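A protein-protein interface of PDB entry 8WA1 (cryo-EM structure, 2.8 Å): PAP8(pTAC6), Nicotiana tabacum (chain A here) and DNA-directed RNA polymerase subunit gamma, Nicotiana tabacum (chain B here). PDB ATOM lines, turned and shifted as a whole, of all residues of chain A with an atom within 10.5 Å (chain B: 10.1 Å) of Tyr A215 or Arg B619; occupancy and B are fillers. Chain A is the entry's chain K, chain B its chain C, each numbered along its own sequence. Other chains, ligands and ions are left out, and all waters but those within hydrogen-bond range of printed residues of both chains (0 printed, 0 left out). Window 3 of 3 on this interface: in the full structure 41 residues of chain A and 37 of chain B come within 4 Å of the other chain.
Tyr A215 touches just one residue of chain B: Arg B619 (2.8 Å).
Arg B619 touches just one residue of chain A: Tyr A215.
No residue of chain A comes within 4 Å of Asp B617.
Of chain A, only Tyr A200 and Ser A217 come within 4 Å of Gln B618.
Val B620 touches just one residue of chain A: Val A202 (3.5 Å).
Of the printed residues of chain B, Tyr A200 touches Gln B618, Tyr B645 and Ile B647.
Of the printed residues of chain B, Val A202 touches Val B620.
Of the printed residues of chain A, Ile B647 touches Tyr A200 (3.5 Å).
Of the printed residues of chain B, Ser A217 touches Gln B618.
Tyr B670 touches none of the printed residues of chain A.
The nearest residue of chain A that does not touch Arg B619 is Val A202 (4.3 Å).
Hydrophobic or aromatic side chains of chain B within 4 Å of the printed part of chain A: Tyr B645 and Ile B647.
Hydrophobic or aromatic side chains of chain A that line the printed part of chain B: Tyr A200, Val A202 and Tyr A215.
Among the printed residues, 6 pairs touch across the chains.
Among the printed residues, no Asp or Glu carboxylate lies within 4 Å of a Lys or Arg side-chain nitrogen of the other chain.
OH of Tyr B670 is in hydrogen-bond range of NH1 of Arg B619 (3.4 Å).
CG of Tyr A200 touches OE1 of Gln B618, 3.9 Å away.
Tyr B645 touches Tyr A200 (OH to CD2, 3.8 Å).
Ile B647 touches Tyr A200.
CG2 of Val A202 touches O of Val B620, at 3.5 Å.
Ser A217 touches Gln B618 (OG to O, 3.6 Å).
The side-chain hydroxyl (OH) of Tyr A215 is in hydrogen-bond range of the guanidinium group (NE) of Arg B619 (2.8 Å).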
ATOM      1  N   TYR A 200      14.922 -37.468  -4.109  1.00  0.00           N
ATOM      2  CA  TYR A 200      14.374 -36.595  -5.140  1.00  0.00           C
ATOM      3  C   TYR A 200      15.471 -35.691  -5.688  1.00  0.00           C
ATOM      4  O   TYR A 200      16.194 -35.046  -4.921  1.00  0.00           O
ATOM      5  CB  TYR A 200      13.227 -35.757  -4.582  1.00  0.00           C
ATOM      6  CG  TYR A 200      11.994 -36.552  -4.217  1.00  0.00           C
ATOM      7  CD1 TYR A 200      10.996 -36.792  -5.153  1.00  0.00           C
ATOM      8  CD2 TYR A 200      11.823 -37.056  -2.936  1.00  0.00           C
ATOM      9  CE1 TYR A 200       9.865 -37.514  -4.823  1.00  0.00           C
ATOM     10  CE2 TYR A 200      10.696 -37.780  -2.597  1.00  0.00           C
ATOM     11  CZ  TYR A 200       9.721 -38.006  -3.544  1.00  0.00           C
ATOM     12  OH  TYR A 200       8.597 -38.726  -3.210  1.00  0.00           O
ATOM     13  N   ASN A 201      15.595 -35.642  -7.012  1.00  0.00           N
ATOM     14  CA  ASN A 201      16.565 -34.781  -7.685  1.00  0.00           C
ATOM     15  C   ASN A 201      15.811 -33.609  -8.302  1.00  0.00           C
ATOM     16  O   ASN A 201      15.242 -33.724  -9.391  1.00  0.00           O
ATOM     17  CB  ASN A 201      17.348 -35.557  -8.737  1.00  0.00           C
ATOM     18  CG  ASN A 201      18.374 -34.698  -9.449  1.00  0.00           C
ATOM     19  OD1 ASN A 201      18.867 -33.714  -8.897  1.00  0.00           O
ATOM     20  ND2 ASN A 201      18.700 -35.065 -10.683  1.00  0.00           N
ATOM     21  N   VAL A 202      15.810 -32.477  -7.605  1.00  0.00           N
ATOM     22  CA  VAL A 202      15.169 -31.256  -8.078  1.00  0.00           C
ATOM     23  C   VAL A 202      16.243 -30.404  -8.739  1.00  0.00           C
ATOM     24  O   VAL A 202      17.080 -29.802  -8.058  1.00  0.00           O
ATOM     25  CB  VAL A 202      14.479 -30.500  -6.937  1.00  0.00           C
ATOM     26  CG1 VAL A 202      13.815 -29.237  -7.465  1.00  0.00           C
ATOM     27  CG2 VAL A 202      13.462 -31.394  -6.246  1.00  0.00           C
ATOM     28  N   THR A 203      16.223 -30.349 -10.067  1.00  0.00           N
ATOM     29  CA  THR A 203      17.218 -29.616 -10.829  1.00  0.00           C
ATOM     30  C   THR A 203      16.644 -28.279 -11.291  1.00  0.00           C
ATOM     31  O   THR A 203      15.514 -27.906 -10.965  1.00  0.00           O
ATOM     32  CB  THR A 203      17.701 -30.449 -12.018  1.00  0.00           C
ATOM     33  OG1 THR A 203      16.597 -30.730 -12.886  1.00  0.00           O
ATOM     34  CG2 THR A 203      18.304 -31.759 -11.536  1.00  0.00           C
ATOM     35  N   GLU A 204      17.444 -27.545 -12.061  1.00  0.00           N
ATOM     36  CA  GLU A 204      17.066 -26.237 -12.592  1.00  0.00           C
ATOM     37  C   GLU A 204      17.311 -26.242 -14.094  1.00  0.00           C
ATOM     38  O   GLU A 204      18.394 -25.863 -14.562  1.00  0.00           O
ATOM     39  CB  GLU A 204      17.842 -25.113 -11.903  1.00  0.00           C
ATOM     40  CG  GLU A 204      17.681 -25.073 -10.388  1.00  0.00           C
ATOM     41  CD  GLU A 204      16.275 -24.704  -9.945  1.00  0.00           C
ATOM     42  OE1 GLU A 204      15.496 -24.187 -10.775  1.00  0.00           O
ATOM     43  OE2 GLU A 204      15.948 -24.929  -8.761  1.00  0.00           O
ATOM     44  N   PRO A 205      16.328 -26.672 -14.879  1.00  0.00           N
ATOM     45  CA  PRO A 205      16.511 -26.755 -16.332  1.00  0.00           C
ATOM     46  C   PRO A 205      16.664 -25.376 -16.945  1.00  0.00           C
ATOM     47  O   PRO A 205      16.038 -24.408 -16.487  1.00  0.00           O
ATOM     48  CB  PRO A 205      15.223 -27.440 -16.810  1.00  0.00           C
ATOM     49  CG  PRO A 205      14.219 -27.111 -15.760  1.00  0.00           C
ATOM     50  CD  PRO A 205      14.979 -27.096 -14.466  1.00  0.00           C
ATOM     51  N   PRO A 206      17.498 -25.244 -17.974  1.00  0.00           N
ATOM     52  CA  PRO A 206      17.667 -23.941 -18.631  1.00  0.00           C
ATOM     53  C   PRO A 206      16.378 -23.492 -19.303  1.00  0.00           C
ATOM     54  O   PRO A 206      15.648 -24.295 -19.887  1.00  0.00           O
ATOM     55  CB  PRO A 206      18.777 -24.201 -19.656  1.00  0.00           C
ATOM     56  CG  PRO A 206      19.472 -25.434 -19.168  1.00  0.00           C
ATOM     57  CD  PRO A 206      18.410 -26.260 -18.521  1.00  0.00           C
ATOM     58  N   ILE A 207      16.102 -22.194 -19.214  1.00  0.00           N
ATOM     59  CA  ILE A 207      14.889 -21.616 -19.782  1.00  0.00           C
ATOM     60  C   ILE A 207      15.226 -21.060 -21.162  1.00  0.00           C
ATOM     61  O   ILE A 207      15.949 -20.069 -21.285  1.00  0.00           O
ATOM     62  CB  ILE A 207      14.306 -20.530 -18.872  1.00  0.00           C
ATOM     63  CG1 ILE A 207      14.056 -21.091 -17.473  1.00  0.00           C
ATOM     64  CG2 ILE A 207      13.017 -19.984 -19.462  1.00  0.00           C
ATOM     65  CD1 ILE A 207      13.487 -20.081 -16.510  1.00  0.00           C
ATOM     66  N   ARG A 211       7.190 -19.914 -21.678  1.00  0.00           N
ATOM     67  CA  ARG A 211       6.571 -20.709 -20.625  1.00  0.00           C
ATOM     68  C   ARG A 211       7.361 -21.973 -20.308  1.00  0.00           C
ATOM     69  O   ARG A 211       6.773 -22.977 -19.891  1.00  0.00           O
ATOM     70  CB  ARG A 211       5.134 -21.060 -21.009  1.00  0.00           C
ATOM     71  CG  ARG A 211       5.002 -21.739 -22.358  1.00  0.00           C
ATOM     72  CD  ARG A 211       3.564 -21.711 -22.834  1.00  0.00           C
ATOM     73  NE  ARG A 211       3.025 -20.355 -22.835  1.00  0.00           N
ATOM     74  CZ  ARG A 211       3.224 -19.471 -23.806  1.00  0.00           C
ATOM     75  NH1 ARG A 211       3.955 -19.799 -24.863  1.00  0.00           N
ATOM     76  NH2 ARG A 211       2.695 -18.259 -23.721  1.00  0.00           N
ATOM     77  N   ASP A 212       8.676 -21.943 -20.501  1.00  0.00           N
ATOM     78  CA  ASP A 212       9.506 -23.091 -20.176  1.00  0.00           C
ATOM     79  C   ASP A 212       9.448 -23.360 -18.672  1.00  0.00           C
ATOM     80  O   ASP A 212       9.420 -22.415 -17.875  1.00  0.00           O
ATOM     81  CB  ASP A 212      10.950 -22.841 -20.617  1.00  0.00           C
ATOM     82  CG  ASP A 212      11.759 -24.117 -20.727  1.00  0.00           C
ATOM     83  OD1 ASP A 212      11.506 -24.906 -21.663  1.00  0.00           O
ATOM     84  OD2 ASP A 212      12.651 -24.330 -19.880  1.00  0.00           O
ATOM     85  N   PRO A 213       9.416 -24.625 -18.252  1.00  0.00           N
ATOM     86  CA  PRO A 213       9.281 -24.922 -16.820  1.00  0.00           C
ATOM     87  C   PRO A 213      10.447 -24.373 -16.012  1.00  0.00           C
ATOM     88  O   PRO A 213      11.586 -24.320 -16.480  1.00  0.00           O
ATOM     89  CB  PRO A 213       9.243 -26.455 -16.778  1.00  0.00           C
ATOM     90  CG  PRO A 213       8.774 -26.857 -18.133  1.00  0.00           C
ATOM     91  CD  PRO A 213       9.348 -25.843 -19.077  1.00  0.00           C
ATOM     92  N   MET A 214      10.144 -23.962 -14.780  1.00  0.00           N
ATOM     93  CA  MET A 214      11.140 -23.427 -13.864  1.00  0.00           C
ATOM     94  C   MET A 214      11.910 -24.508 -13.119  1.00  0.00           C
ATOM     95  O   MET A 214      12.991 -24.223 -12.592  1.00  0.00           O
ATOM     96  CB  MET A 214      10.471 -22.496 -12.845  1.00  0.00           C
ATOM     97  CG  MET A 214       9.883 -21.230 -13.443  1.00  0.00           C
ATOM     98  SD  MET A 214      11.139 -19.987 -13.792  1.00  0.00           S
ATOM     99  CE  MET A 214      11.790 -19.700 -12.150  1.00  0.00           C
ATOM    100  N   TYR A 215      11.389 -25.732 -13.061  1.00  0.00           N
ATOM    101  CA  TYR A 215      12.025 -26.793 -12.295  1.00  0.00           C
ATOM    102  C   TYR A 215      11.682 -28.141 -12.906  1.00  0.00           C
ATOM    103  O   TYR A 215      10.722 -28.269 -13.671  1.00  0.00           O
ATOM    104  CB  TYR A 215      11.593 -26.760 -10.824  1.00  0.00           C
ATOM    105  CG  TYR A 215      10.126 -27.051 -10.603  1.00  0.00           C
ATOM    106  CD1 TYR A 215       9.171 -26.052 -10.733  1.00  0.00           C
ATOM    107  CD2 TYR A 215       9.695 -28.327 -10.262  1.00  0.00           C
ATOM    108  CE1 TYR A 215       7.828 -26.315 -10.531  1.00  0.00           C
ATOM    109  CE2 TYR A 215       8.357 -28.600 -10.059  1.00  0.00           C
ATOM    110  CZ  TYR A 215       7.427 -27.590 -10.194  1.00  0.00           C
ATOM    111  OH  TYR A 215       6.093 -27.858  -9.992  1.00  0.00           O
ATOM    112  N   LYS A 216      12.482 -29.146 -12.558  1.00  0.00           N
ATOM    113  CA  LYS A 216      12.262 -30.523 -12.976  1.00  0.00           C
ATOM    114  C   LYS A 216      12.511 -31.433 -11.784  1.00  0.00           C
ATOM    115  O   LYS A 216      13.596 -31.404 -11.195  1.00  0.00           O
ATOM    116  CB  LYS A 216      13.180 -30.903 -14.143  1.00  0.00           C
ATOM    117  CG  LYS A 216      12.896 -32.267 -14.743  1.00  0.00           C
ATOM    118  CD  LYS A 216      13.814 -32.548 -15.923  1.00  0.00           C
ATOM    119  CE  LYS A 216      13.473 -33.871 -16.584  1.00  0.00           C
ATOM    120  NZ  LYS A 216      14.350 -34.148 -17.755  1.00  0.00           N
ATOM    121  N   SER A 217      11.511 -32.237 -11.433  1.00  0.00           N
ATOM    122  CA  SER A 217      11.573 -33.114 -10.271  1.00  0.00           C
ATOM    123  C   SER A 217      11.538 -34.566 -10.724  1.00  0.00           C
ATOM    124  O   SER A 217      10.696 -34.946 -11.543  1.00  0.00           O
ATOM    125  CB  SER A 217      10.417 -32.830  -9.310  1.00  0.00           C
ATOM    126  OG  SER A 217      10.483 -33.673  -8.173  1.00  0.00           O
ATOM    127  N   GLU A 218      12.452 -35.373 -10.187  1.00  0.00           N
ATOM    128  CA  GLU A 218      12.539 -36.791 -10.511  1.00  0.00           C
ATOM    129  C   GLU A 218      12.619 -37.592  -9.220  1.00  0.00           C
ATOM    130  O   GLU A 218      13.335 -37.208  -8.290  1.00  0.00           O
ATOM    131  CB  GLU A 218      13.754 -37.086 -11.398  1.00  0.00           C
ATOM    132  CG  GLU A 218      13.722 -36.389 -12.750  1.00  0.00           C
ATOM    133  CD  GLU A 218      12.577 -36.860 -13.627  1.00  0.00           C
ATOM    134  OE1 GLU A 218      12.147 -38.024 -13.473  1.00  0.00           O
ATOM    135  OE2 GLU A 218      12.105 -36.068 -14.469  1.00  0.00           O
ATOM    136  N   TRP B 614       2.504 -29.478   2.757  1.00  0.00           N
ATOM    137  CA  TRP B 614       2.458 -29.112   1.349  1.00  0.00           C
ATOM    138  C   TRP B 614       1.471 -30.005   0.612  1.00  0.00           C
ATOM    139  O   TRP B 614       1.264 -31.163   0.992  1.00  0.00           O
ATOM    140  CB  TRP B 614       3.838 -29.217   0.697  1.00  0.00           C
ATOM    141  CG  TRP B 614       4.383 -27.898   0.257  1.00  0.00           C
ATOM    142  CD1 TRP B 614       4.090 -26.675   0.784  1.00  0.00           C
ATOM    143  CD2 TRP B 614       5.303 -27.663  -0.814  1.00  0.00           C
ATOM    144  NE1 TRP B 614       4.778 -25.692   0.114  1.00  0.00           N
ATOM    145  CE2 TRP B 614       5.530 -26.274  -0.873  1.00  0.00           C
ATOM    146  CE3 TRP B 614       5.961 -28.492  -1.727  1.00  0.00           C
ATOM    147  CZ2 TRP B 614       6.385 -25.696  -1.806  1.00  0.00           C
ATOM    148  CZ3 TRP B 614       6.809 -27.917  -2.652  1.00  0.00           C
ATOM    149  CH2 TRP B 614       7.014 -26.533  -2.686  1.00  0.00           C
ATOM    150  N   ARG B 615       0.861 -29.462  -0.443  1.00  0.00           N
ATOM    151  CA  ARG B 615      -0.149 -30.183  -1.216  1.00  0.00           C
ATOM    152  C   ARG B 615       0.495 -30.773  -2.468  1.00  0.00           C
ATOM    153  O   ARG B 615       0.278 -30.314  -3.590  1.00  0.00           O
ATOM    154  CB  ARG B 615      -1.314 -29.262  -1.564  1.00  0.00           C
ATOM    155  CG  ARG B 615      -2.036 -28.680  -0.361  1.00  0.00           C
ATOM    156  CD  ARG B 615      -2.524 -29.779   0.567  1.00  0.00           C
ATOM    157  NE  ARG B 615      -3.425 -29.266   1.594  1.00  0.00           N
ATOM    158  CZ  ARG B 615      -3.026 -28.779   2.764  1.00  0.00           C
ATOM    159  NH1 ARG B 615      -1.734 -28.731   3.060  1.00  0.00           N
ATOM    160  NH2 ARG B 615      -3.918 -28.335   3.637  1.00  0.00           N
ATOM    161  N   LEU B 616       1.286 -31.826  -2.255  1.00  0.00           N
ATOM    162  CA  LEU B 616       1.800 -32.688  -3.324  1.00  0.00           C
ATOM    163  C   LEU B 616       2.415 -31.885  -4.472  1.00  0.00           C
ATOM    164  O   LEU B 616       1.935 -31.906  -5.607  1.00  0.00           O
ATOM    165  CB  LEU B 616       0.697 -33.614  -3.839  1.00  0.00           C
ATOM    166  CG  LEU B 616       0.000 -34.474  -2.782  1.00  0.00           C
ATOM    167  CD1 LEU B 616      -1.121 -35.293  -3.404  1.00  0.00           C
ATOM    168  CD2 LEU B 616       1.002 -35.376  -2.079  1.00  0.00           C
ATOM    169  N   ASP B 617       3.499 -31.168  -4.169  1.00  0.00           N
ATOM    170  CA  ASP B 617       4.223 -30.417  -5.184  1.00  0.00           C
ATOM    171  C   ASP B 617       5.681 -30.822  -5.337  1.00  0.00           C
ATOM    172  O   ASP B 617       6.150 -30.926  -6.475  1.00  0.00           O
ATOM    173  CB  ASP B 617       4.163 -28.910  -4.886  1.00  0.00           C
ATOM    174  CG  ASP B 617       2.769 -28.338  -5.050  1.00  0.00           C
ATOM    175  OD1 ASP B 617       1.993 -28.887  -5.860  1.00  0.00           O
ATOM    176  OD2 ASP B 617       2.452 -27.337  -4.372  1.00  0.00           O
ATOM    177  N   GLN B 618       6.398 -31.064  -4.239  1.00  0.00           N
ATOM    178  CA  GLN B 618       7.801 -31.479  -4.267  1.00  0.00           C
ATOM    179  C   GLN B 618       8.647 -30.548  -5.137  1.00  0.00           C
ATOM    180  O   GLN B 618       9.300 -30.969  -6.095  1.00  0.00           O
ATOM    181  CB  GLN B 618       7.934 -32.930  -4.730  1.00  0.00           C
ATOM    182  CG  GLN B 618       8.333 -33.886  -3.620  1.00  0.00           C
ATOM    183  CD  GLN B 618       9.642 -33.493  -2.960  1.00  0.00           C
ATOM    184  OE1 GLN B 618      10.550 -32.980  -3.613  1.00  0.00           O
ATOM    185  NE2 GLN B 618       9.739 -33.727  -1.657  1.00  0.00           N
ATOM    186  N   ARG B 619       8.636 -29.263  -4.786  1.00  0.00           N
ATOM    187  CA  ARG B 619       9.401 -28.246  -5.495  1.00  0.00           C
ATOM    188  C   ARG B 619      10.577 -27.734  -4.672  1.00  0.00           C
ATOM    189  O   ARG B 619      11.259 -26.792  -5.087  1.00  0.00           O
ATOM    190  CB  ARG B 619       8.494 -27.083  -5.893  1.00  0.00           C
ATOM    191  CG  ARG B 619       7.273 -27.484  -6.699  1.00  0.00           C
ATOM    192  CD  ARG B 619       6.380 -26.280  -6.943  1.00  0.00           C
ATOM    193  NE  ARG B 619       5.179 -26.625  -7.694  1.00  0.00           N
ATOM    194  CZ  ARG B 619       4.204 -25.766  -7.971  1.00  0.00           C
ATOM    195  NH1 ARG B 619       4.288 -24.510  -7.554  1.00  0.00           N
ATOM    196  NH2 ARG B 619       3.144 -26.162  -8.662  1.00  0.00           N
ATOM    197  N   VAL B 620      10.828 -28.338  -3.515  1.00  0.00           N
ATOM    198  CA  VAL B 620      11.885 -27.883  -2.619  1.00  0.00           C
ATOM    199  C   VAL B 620      13.229 -28.380  -3.139  1.00  0.00           C
ATOM    200  O   VAL B 620      13.443 -29.587  -3.287  1.00  0.00           O
ATOM    201  CB  VAL B 620      11.633 -28.360  -1.182  1.00  0.00           C
ATOM    202  CG1 VAL B 620      11.116 -29.791  -1.174  1.00  0.00           C
ATOM    203  CG2 VAL B 620      12.905 -28.254  -0.366  1.00  0.00           C
ATOM    204  N   ILE B 621      14.134 -27.446  -3.426  1.00  0.00           N
ATOM    205  CA  ILE B 621      15.470 -27.814  -3.877  1.00  0.00           C
ATOM    206  C   ILE B 621      16.283 -28.316  -2.692  1.00  0.00           C
ATOM    207  O   ILE B 621      16.361 -27.658  -1.646  1.00  0.00           O
ATOM    208  CB  ILE B 621      16.153 -26.626  -4.571  1.00  0.00           C
ATOM    209  CG1 ILE B 621      17.640 -26.916  -4.794  1.00  0.00           C
ATOM    210  CG2 ILE B 621      15.954 -25.344  -3.772  1.00  0.00           C
ATOM    211  CD1 ILE B 621      18.379 -25.802  -5.503  1.00  0.00           C
ATOM    212  N   ALA B 622      16.882 -29.495  -2.846  1.00  0.00           N
ATOM    213  CA  ALA B 622      17.664 -30.102  -1.779  1.00  0.00           C
ATOM    214  C   ALA B 622      18.688 -31.042  -2.399  1.00  0.00           C
ATOM    215  O   ALA B 622      18.673 -31.304  -3.604  1.00  0.00           O
ATOM    216  CB  ALA B 622      16.768 -30.843  -0.782  1.00  0.00           C
ATOM    217  N   TYR B 645      12.409 -32.562   4.999  1.00  0.00           N
ATOM    218  CA  TYR B 645      10.984 -32.806   4.821  1.00  0.00           C
ATOM    219  C   TYR B 645      10.646 -34.233   5.226  1.00  0.00           C
ATOM    220  O   TYR B 645      11.507 -35.116   5.255  1.00  0.00           O
ATOM    221  CB  TYR B 645      10.544 -32.538   3.377  1.00  0.00           C
ATOM    222  CG  TYR B 645      11.436 -33.160   2.328  1.00  0.00           C
ATOM    223  CD1 TYR B 645      12.525 -32.467   1.817  1.00  0.00           C
ATOM    224  CD2 TYR B 645      11.185 -34.436   1.842  1.00  0.00           C
ATOM    225  CE1 TYR B 645      13.343 -33.028   0.857  1.00  0.00           C
ATOM    226  CE2 TYR B 645      11.997 -35.004   0.881  1.00  0.00           C
ATOM    227  CZ  TYR B 645      13.075 -34.298   0.393  1.00  0.00           C
ATOM    228  OH  TYR B 645      13.888 -34.862  -0.565  1.00  0.00           O
ATOM    229  N   ILE B 647       7.779 -37.325   4.403  1.00  0.00           N
ATOM    230  CA  ILE B 647       6.846 -37.789   3.377  1.00  0.00           C
ATOM    231  C   ILE B 647       6.225 -39.084   3.889  1.00  0.00           C
ATOM    232  O   ILE B 647       6.840 -40.153   3.846  1.00  0.00           O
ATOM    233  CB  ILE B 647       7.525 -37.989   2.021  1.00  0.00           C
ATOM    234  CG1 ILE B 647       8.092 -36.661   1.517  1.00  0.00           C
ATOM    235  CG2 ILE B 647       6.544 -38.566   1.014  1.00  0.00           C
ATOM    236  CD1 ILE B 647       8.806 -36.768   0.194  1.00  0.00           C
ATOM    237  N   ILE B 658       2.763 -34.651   3.117  1.00  0.00           N
ATOM    238  CA  ILE B 658       4.108 -34.117   2.940  1.00  0.00           C
ATOM    239  C   ILE B 658       4.249 -32.896   3.837  1.00  0.00           C
ATOM    240  O   ILE B 658       3.434 -31.971   3.763  1.00  0.00           O
ATOM    241  CB  ILE B 658       4.395 -33.744   1.474  1.00  0.00           C
ATOM    242  CG1 ILE B 658       4.377 -34.990   0.588  1.00  0.00           C
ATOM    243  CG2 ILE B 658       5.734 -33.029   1.360  1.00  0.00           C
ATOM    244  CD1 ILE B 658       4.645 -34.703  -0.875  1.00  0.00           C
ATOM    245  N   ILE B 660       7.064 -29.985   5.083  1.00  0.00           N
ATOM    246  CA  ILE B 660       8.347 -29.351   4.847  1.00  0.00           C
ATOM    247  C   ILE B 660       8.821 -28.711   6.144  1.00  0.00           C
ATOM    248  O   ILE B 660       8.056 -28.075   6.873  1.00  0.00           O
ATOM    249  CB  ILE B 660       8.267 -28.304   3.710  1.00  0.00           C
ATOM    250  CG1 ILE B 660       7.594 -28.904   2.474  1.00  0.00           C
ATOM    251  CG2 ILE B 660       9.651 -27.783   3.362  1.00  0.00           C
ATOM    252  CD1 ILE B 660       8.353 -30.057   1.861  1.00  0.00           C
ATOM    253  N   TYR B 670       8.536 -17.077  -0.573  1.00  0.00           N
ATOM    254  CA  TYR B 670       7.775 -17.826  -1.567  1.00  0.00           C
ATOM    255  C   TYR B 670       6.358 -17.282  -1.702  1.00  0.00           C
ATOM    256  O   TYR B 670       5.860 -17.104  -2.821  1.00  0.00           O
ATOM    257  CB  TYR B 670       7.755 -19.308  -1.195  1.00  0.00           C
ATOM    258  CG  TYR B 670       6.984 -20.181  -2.157  1.00  0.00           C
ATOM    259  CD1 TYR B 670       7.571 -20.647  -3.326  1.00  0.00           C
ATOM    260  CD2 TYR B 670       5.673 -20.550  -1.891  1.00  0.00           C
ATOM    261  CE1 TYR B 670       6.871 -21.449  -4.206  1.00  0.00           C
ATOM    262  CE2 TYR B 670       4.965 -21.351  -2.764  1.00  0.00           C
ATOM    263  CZ  TYR B 670       5.568 -21.798  -3.920  1.00  0.00           C
ATOM    264  OH  TYR B 670       4.866 -22.596  -4.791  1.00  0.00           O
ATOM    265  N   GLU B 674       4.713 -15.569  -5.045  1.00  0.00           N
ATOM    266  CA  GLU B 674       3.524 -16.184  -5.625  1.00  0.00           C
ATOM    267  C   GLU B 674       2.346 -15.219  -5.616  1.00  0.00           C
ATOM    268  O   GLU B 674       1.594 -15.139  -6.594  1.00  0.00           O
ATOM    269  CB  GLU B 674       3.183 -17.469  -4.868  1.00  0.00           C
ATOM    270  CG  GLU B 674       2.368 -18.492  -5.654  1.00  0.00           C
ATOM    271  CD  GLU B 674       0.890 -18.155  -5.725  1.00  0.00           C
ATOM    272  OE1 GLU B 674       0.456 -17.584  -6.746  1.00  0.00           O
ATOM    273  OE2 GLU B 674       0.162 -18.465  -4.759  1.00  0.00           O
ATOM    274  N   ILE B 677       2.731 -12.599  -8.345  1.00  0.00           N
ATOM    275  CA  ILE B 677       2.335 -13.146  -9.640  1.00  0.00           C
ATOM    276  C   ILE B 677       0.816 -13.241  -9.743  1.00  0.00           C
ATOM    277  O   ILE B 677       0.219 -12.847 -10.757  1.00  0.00           O
ATOM    278  CB  ILE B 677       3.001 -14.516  -9.867  1.00  0.00           C
ATOM    279  CG1 ILE B 677       4.521 -14.384  -9.810  1.00  0.00           C
ATOM    280  CG2 ILE B 677       2.567 -15.100 -11.200  1.00  0.00           C
ATOM    281  CD1 ILE B 677       5.254 -15.701  -9.920  1.00  0.00           C
